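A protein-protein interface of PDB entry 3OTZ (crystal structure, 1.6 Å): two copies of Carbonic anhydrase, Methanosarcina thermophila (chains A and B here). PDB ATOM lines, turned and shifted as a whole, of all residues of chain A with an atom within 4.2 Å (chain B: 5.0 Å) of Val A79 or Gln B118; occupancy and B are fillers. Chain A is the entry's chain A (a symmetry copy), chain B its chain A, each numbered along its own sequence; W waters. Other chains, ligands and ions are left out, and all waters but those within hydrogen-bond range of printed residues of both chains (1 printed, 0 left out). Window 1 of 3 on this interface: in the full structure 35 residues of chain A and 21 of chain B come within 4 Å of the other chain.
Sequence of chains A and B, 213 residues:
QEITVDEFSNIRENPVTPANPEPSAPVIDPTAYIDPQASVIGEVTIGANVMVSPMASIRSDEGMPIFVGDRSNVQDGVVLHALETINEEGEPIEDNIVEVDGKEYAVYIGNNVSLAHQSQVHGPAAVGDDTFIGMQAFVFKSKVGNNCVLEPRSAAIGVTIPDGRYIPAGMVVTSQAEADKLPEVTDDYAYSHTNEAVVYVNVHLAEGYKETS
OD2 of Asp B76 sits at hydrogen-bond distance from OG of Ser A57, at 2.7 Å.
O of His B117 sits at hydrogen-bond distance from NE2 of Gln A120 (3.3 Å).
O of Gly A77 sits at hydrogen-bond distance from NE2 of Gln B118 (2.9 Å).
The backbone carbonyl oxygen (O) of Gln A118 is in hydrogen-bond range of the side-chain amide nitrogen (NE2) of Gln B118, 3.3 Å away.
O of Ser A119 sits at hydrogen-bond distance from NE2 of Gln B118 (3.2 Å).
The side-chain amide oxygen (OE1) of Gln B118 sits at hydrogen-bond distance from the side-chain amide nitrogen (NE2) of Gln A120 (2.9 Å).
OD1 of Asp B76 lies within hydrogen-bond range of ND1 of His B117, 2.8 Å away.
The backbone carbonyl oxygen of Asp B76 lies within hydrogen-bond range of the backbone NH of Gln B118 (2.9 Å).
N of Gln B136 is in hydrogen-bond range of O of His B117 (3.0 Å).
N of Ser A57 is in hydrogen-bond range of O of Val A78 (2.9 Å).
The backbone NH (N) of Val A79 lies within hydrogen-bond range of the backbone carbonyl oxygen (O) of Ser A119, 3.3 Å away.
O of Val A79 lies within hydrogen-bond range of N of Val A121, at 3.2 Å.
Among the printed residues, pairs that only touch across the chains: Val A79 with His B117, Val A79 with Gln B118, Gln A118 with Gln B136 and Gln A120 with Gln B136.
Printed residues of chain B within 4 Å of Val A79: His B117 and Gln B118.
Gln B118 touches five residues of chain A.
Printed residues of chain B within 4 Å of Ser A57: Asp B76 (2.7 Å).
Printed residues of chain A within 4 Å of His B117: Val A79 and Gln A120.
The nearest printed residue of chain A that does not touch Gln B118 is Val A78 (4.3 Å).
Of the 10 printed residues of chain B, 4 touch a printed residue of chain A.
Hydrophobic or aromatic side chains of chain B within 4 Å of the printed part of chain A: His B117.
Printed residues of chain A that touch a printed residue of chain B: Ser A57, Gly A77, Val A79, Gln A118, Ser A119 and Gln A120.
Hydrophobic or aromatic side chains of chain A that line the printed part of chain B: Val A79.
Along chain A the printed residues that touch a printed residue of chain B span positions 57 to 120.
Among the printed residues, 10 pairs touch across the chains.
Among the printed residues, no Asp or Glu carboxylate lies within 4 Å of a Lys or Arg side-chain nitrogen of the other chain.
Gly A77 touches Gln B118, but with the chains exchanged Gln A118 does not touch Gly B77 (8.2 Å).
Gln A118 touches its own counterpart, Gln B118.
Ser A119 touches Gln B118, but with the chains exchanged Gln A118 does not touch Ser B119 (9.1 Å).
Gln A120 touches Gln B118, but with the chains exchanged Gln A118 does not touch Gln B120 (8.8 Å).
Of the 10 pairs that touch across the chains among the printed residues, 1 has its exchanged pair printed and touching as well.
Water W1 lies within hydrogen-bond range of O of Gln A118 (2.8 Å) and NE2 of Gln B136 (3.5 Å).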
ATOM      1  N   SER A  57       6.817  -3.589  26.750  1.00  0.00           N
ATOM      2  CA  SER A  57       5.671  -2.807  26.305  1.00  0.00           C
ATOM      3  C   SER A  57       4.872  -2.444  27.529  1.00  0.00           C
ATOM      4  O   SER A  57       4.333  -3.328  28.167  1.00  0.00           O
ATOM      5  CB  SER A  57       4.834  -3.588  25.294  1.00  0.00           C
ATOM      6  OG  SER A  57       3.756  -2.742  24.844  1.00  0.00           O
ATOM      7  N   GLY A  77      11.110  -7.623  27.012  1.00  0.00           N
ATOM      8  CA  GLY A  77       9.941  -8.414  26.660  1.00  0.00           C
ATOM      9  C   GLY A  77       8.842  -8.391  27.713  1.00  0.00           C
ATOM     10  O   GLY A  77       7.858  -9.136  27.523  1.00  0.00           O
ATOM     11  N   VAL A  78       8.965  -7.609  28.801  1.00  0.00           N
ATOM     12  CA  VAL A  78       7.920  -7.573  29.819  1.00  0.00           C
ATOM     13  C   VAL A  78       6.720  -6.794  29.270  1.00  0.00           C
ATOM     14  O   VAL A  78       6.908  -5.838  28.513  1.00  0.00           O
ATOM     15  CB  VAL A  78       8.451  -6.910  31.086  1.00  0.00           C
ATOM     16  CG1 VAL A  78       7.294  -6.509  32.094  1.00  0.00           C
ATOM     17  CG2 VAL A  78       9.440  -7.892  31.746  1.00  0.00           C
ATOM     18  N   VAL A  79       5.506  -7.269  29.571  1.00  0.00           N
ATOM     19  CA  VAL A  79       4.320  -6.508  29.178  1.00  0.00           C
ATOM     20  C   VAL A  79       3.566  -6.077  30.440  1.00  0.00           C
ATOM     21  O   VAL A  79       3.351  -6.874  31.359  1.00  0.00           O
ATOM     22  CB  VAL A  79       3.402  -7.378  28.321  1.00  0.00           C
ATOM     23  CG1 VAL A  79       2.034  -6.625  28.021  1.00  0.00           C
ATOM     24  CG2 VAL A  79       4.087  -7.732  27.009  1.00  0.00           C
ATOM     25  N   LEU A  80       3.198  -4.789  30.475  1.00  0.00           N
ATOM     26  CA  LEU A  80       2.248  -4.262  31.478  1.00  0.00           C
ATOM     27  C   LEU A  80       1.050  -3.715  30.717  1.00  0.00           C
ATOM     28  O   LEU A  80       1.208  -2.870  29.838  1.00  0.00           O
ATOM     29  CB  LEU A  80       2.869  -3.115  32.309  1.00  0.00           C
ATOM     30  CG  LEU A  80       4.140  -3.478  33.110  1.00  0.00           C
ATOM     31  CD1 LEU A  80       4.659  -2.247  33.893  1.00  0.00           C
ATOM     32  CD2 LEU A  80       3.859  -4.618  34.041  1.00  0.00           C
ATOM     33  N   GLN A 118      10.548 -11.229  30.121  1.00  0.00           N
ATOM     34  CA  GLN A 118       9.371 -11.932  29.581  1.00  0.00           C
ATOM     35  C   GLN A 118       8.258 -12.155  30.599  1.00  0.00           C
ATOM     36  O   GLN A 118       7.305 -12.874  30.292  1.00  0.00           O
ATOM     37  CB  GLN A 118       9.746 -13.268  28.914  1.00  0.00           C
ATOM     38  CG  GLN A 118      10.698 -13.104  27.726  1.00  0.00           C
ATOM     39  CD  GLN A 118      11.089 -14.444  27.173  1.00  0.00           C
ATOM     40  OE1 GLN A 118      11.191 -15.399  27.906  1.00  0.00           O
ATOM     41  NE2 GLN A 118      11.344 -14.516  25.857  1.00  0.00           N
ATOM     42  N   SER A 119       8.375 -11.572  31.787  1.00  0.00           N
ATOM     43  CA  SER A 119       7.235 -11.649  32.717  1.00  0.00           C
ATOM     44  C   SER A 119       6.105 -10.717  32.248  1.00  0.00           C
ATOM     45  O   SER A 119       6.252  -9.930  31.301  1.00  0.00           O
ATOM     46  CB  SER A 119       7.669 -11.328  34.172  1.00  0.00           C
ATOM     47  OG  SER A 119       8.123  -9.953  34.282  1.00  0.00           O
ATOM     48  N   GLN A 120       4.968 -10.790  32.936  1.00  0.00           N
ATOM     49  CA  GLN A 120       3.851  -9.913  32.572  1.00  0.00           C
ATOM     50  C   GLN A 120       3.056  -9.660  33.851  1.00  0.00           C
ATOM     51  O   GLN A 120       2.799 -10.583  34.614  1.00  0.00           O
ATOM     52  CB  GLN A 120       2.961 -10.608  31.553  1.00  0.00           C
ATOM     53  CG  GLN A 120       1.627  -9.862  31.289  1.00  0.00           C
ATOM     54  CD  GLN A 120       0.743 -10.462  30.182  1.00  0.00           C
ATOM     55  OE1 GLN A 120      -0.408 -10.035  30.064  1.00  0.00           O
ATOM     56  NE2 GLN A 120       1.249 -11.405  29.371  1.00  0.00           N
ATOM     57  N   VAL A 121       2.663  -8.400  34.062  1.00  0.00           N
ATOM     58  CA  VAL A 121       1.780  -8.072  35.174  1.00  0.00           C
ATOM     59  C   VAL A 121       0.620  -7.392  34.494  1.00  0.00           C
ATOM     60  O   VAL A 121       0.787  -6.371  33.833  1.00  0.00           O
ATOM     61  CB  VAL A 121       2.422  -7.136  36.194  1.00  0.00           C
ATOM     62  CG1 VAL A 121       1.368  -6.723  37.269  1.00  0.00           C
ATOM     63  CG2 VAL A 121       3.642  -7.835  36.833  1.00  0.00           C
ATOM     64  N   ASP B  76       0.299  -7.466  22.569  1.00  0.00           N
ATOM     65  CA  ASP B  76       1.739  -7.144  22.645  1.00  0.00           C
ATOM     66  C   ASP B  76       2.544  -8.434  22.782  1.00  0.00           C
ATOM     67  O   ASP B  76       2.217  -9.281  23.610  1.00  0.00           O
ATOM     68  CB  ASP B  76       2.068  -6.250  23.869  1.00  0.00           C
ATOM     69  CG  ASP B  76       1.067  -5.119  24.080  1.00  0.00           C
ATOM     70  OD1 ASP B  76      -0.108  -5.433  24.297  1.00  0.00           O
ATOM     71  OD2 ASP B  76       1.464  -3.958  24.074  1.00  0.00           O
ATOM     72  N   GLY B  77       3.603  -8.545  21.988  1.00  0.00           N
ATOM     73  CA  GLY B  77       4.501  -9.675  22.171  1.00  0.00           C
ATOM     74  C   GLY B  77       3.970 -10.982  21.598  1.00  0.00           C
ATOM     75  O   GLY B  77       4.640 -12.012  21.816  1.00  0.00           O
ATOM     76  N   VAL B  78       2.812 -10.998  20.912  1.00  0.00           N
ATOM     77  CA  VAL B  78       2.289 -12.241  20.355  1.00  0.00           C
ATOM     78  C   VAL B  78       3.133 -12.632  19.138  1.00  0.00           C
ATOM     79  O   VAL B  78       3.599 -11.752  18.409  1.00  0.00           O
ATOM     80  CB  VAL B  78       0.829 -12.057  19.954  1.00  0.00           C
ATOM     81  CG1 VAL B  78       0.302 -13.227  19.021  1.00  0.00           C
ATOM     82  CG2 VAL B  78      -0.003 -11.969  21.250  1.00  0.00           C
ATOM     83  N   ALA B 116      -4.173 -12.838  23.266  1.00  0.00           N
ATOM     84  CA  ALA B 116      -3.774 -11.918  24.328  1.00  0.00           C
ATOM     85  C   ALA B 116      -2.249 -11.881  24.532  1.00  0.00           C
ATOM     86  O   ALA B 116      -1.498 -12.715  24.009  1.00  0.00           O
ATOM     87  CB  ALA B 116      -4.468 -12.321  25.621  1.00  0.00           C
ATOM     88  N   HIS B 117      -1.814 -10.904  25.316  1.00  0.00           N
ATOM     89  CA  HIS B 117      -0.373 -10.561  25.376  1.00  0.00           C
ATOM     90  C   HIS B 117       0.504 -11.784  25.603  1.00  0.00           C
ATOM     91  O   HIS B 117       0.263 -12.590  26.498  1.00  0.00           O
ATOM     92  CB  HIS B 117      -0.103  -9.597  26.534  1.00  0.00           C
ATOM     93  CG  HIS B 117      -1.140  -8.522  26.712  1.00  0.00           C
ATOM     94  ND1 HIS B 117      -1.103  -7.304  26.060  1.00  0.00           N
ATOM     95  CD2 HIS B 117      -2.230  -8.489  27.515  1.00  0.00           C
ATOM     96  CE1 HIS B 117      -2.125  -6.555  26.471  1.00  0.00           C
ATOM     97  NE2 HIS B 117      -2.832  -7.269  27.337  1.00  0.00           N
ATOM     98  N   GLN B 118       1.560 -11.855  24.792  1.00  0.00           N
ATOM     99  CA  GLN B 118       2.618 -12.875  24.900  1.00  0.00           C
ATOM    100  C   GLN B 118       2.161 -14.285  24.541  1.00  0.00           C
ATOM    101  O   GLN B 118       2.923 -15.230  24.756  1.00  0.00           O
ATOM    102  CB  GLN B 118       3.285 -12.877  26.287  1.00  0.00           C
ATOM    103  CG  GLN B 118       3.968 -11.550  26.631  1.00  0.00           C
ATOM    104  CD  GLN B 118       4.526 -11.589  28.025  1.00  0.00           C
ATOM    105  OE1 GLN B 118       3.969 -12.228  28.886  1.00  0.00           O
ATOM    106  NE2 GLN B 118       5.632 -10.868  28.265  1.00  0.00           N
ATOM    107  N   SER B 119       0.947 -14.433  24.025  1.00  0.00           N
ATOM    108  CA  SER B 119       0.558 -15.765  23.528  1.00  0.00           C
ATOM    109  C   SER B 119       1.279 -16.068  22.204  1.00  0.00           C
ATOM    110  O   SER B 119       1.959 -15.214  21.614  1.00  0.00           O
ATOM    111  CB  SER B 119      -0.982 -15.886  23.377  1.00  0.00           C
ATOM    112  OG  SER B 119      -1.473 -14.972  22.360  1.00  0.00           O
ATOM    113  N   GLN B 120       1.108 -17.294  21.716  1.00  0.00           N
ATOM    114  CA  GLN B 120       1.737 -17.654  20.441  1.00  0.00           C
ATOM    115  C   GLN B 120       0.847 -18.712  19.794  1.00  0.00           C
ATOM    116  O   GLN B 120       0.397 -19.636  20.462  1.00  0.00           O
ATOM    117  CB  GLN B 120       3.117 -18.242  20.695  1.00  0.00           C
ATOM    118  CG  GLN B 120       3.760 -18.874  19.432  1.00  0.00           C
ATOM    119  CD  GLN B 120       5.202 -19.378  19.609  1.00  0.00           C
ATOM    120  OE1 GLN B 120       5.691 -20.064  18.708  1.00  0.00           O
ATOM    121  NE2 GLN B 120       5.888 -19.046  20.715  1.00  0.00           N
ATOM    122  N   GLN B 136       0.051 -15.433  27.539  1.00  0.00           N
ATOM    123  CA  GLN B 136       1.129 -16.450  27.611  1.00  0.00           C
ATOM    124  C   GLN B 136       0.707 -17.849  27.166  1.00  0.00           C
ATOM    125  O   GLN B 136       1.411 -18.803  27.452  1.00  0.00           O
ATOM    126  CB  GLN B 136       1.756 -16.526  29.004  1.00  0.00           C
ATOM    127  CG  GLN B 136       2.417 -15.187  29.416  1.00  0.00           C
ATOM    128  CD  GLN B 136       3.171 -15.269  30.730  1.00  0.00           C
ATOM    129  OE1 GLN B 136       2.978 -16.207  31.497  1.00  0.00           O
ATOM    130  NE2 GLN B 136       4.012 -14.272  31.010  1.00  0.00           N
ATOM    131  N   ALA B 137      -0.445 -17.991  26.527  1.00  0.00           N
ATOM    132  CA  ALA B 137      -0.896 -19.318  26.117  1.00  0.00           C
ATOM    133  C   ALA B 137      -0.195 -19.718  24.820  1.00  0.00           C
ATOM    134  O   ALA B 137       0.453 -18.904  24.174  1.00  0.00           O
ATOM    135  CB  ALA B 137      -2.412 -19.312  25.904  1.00  0.00           C
HETATM  136  O   HOH W   1       6.481 -15.028  28.684  1.00  0.00           O
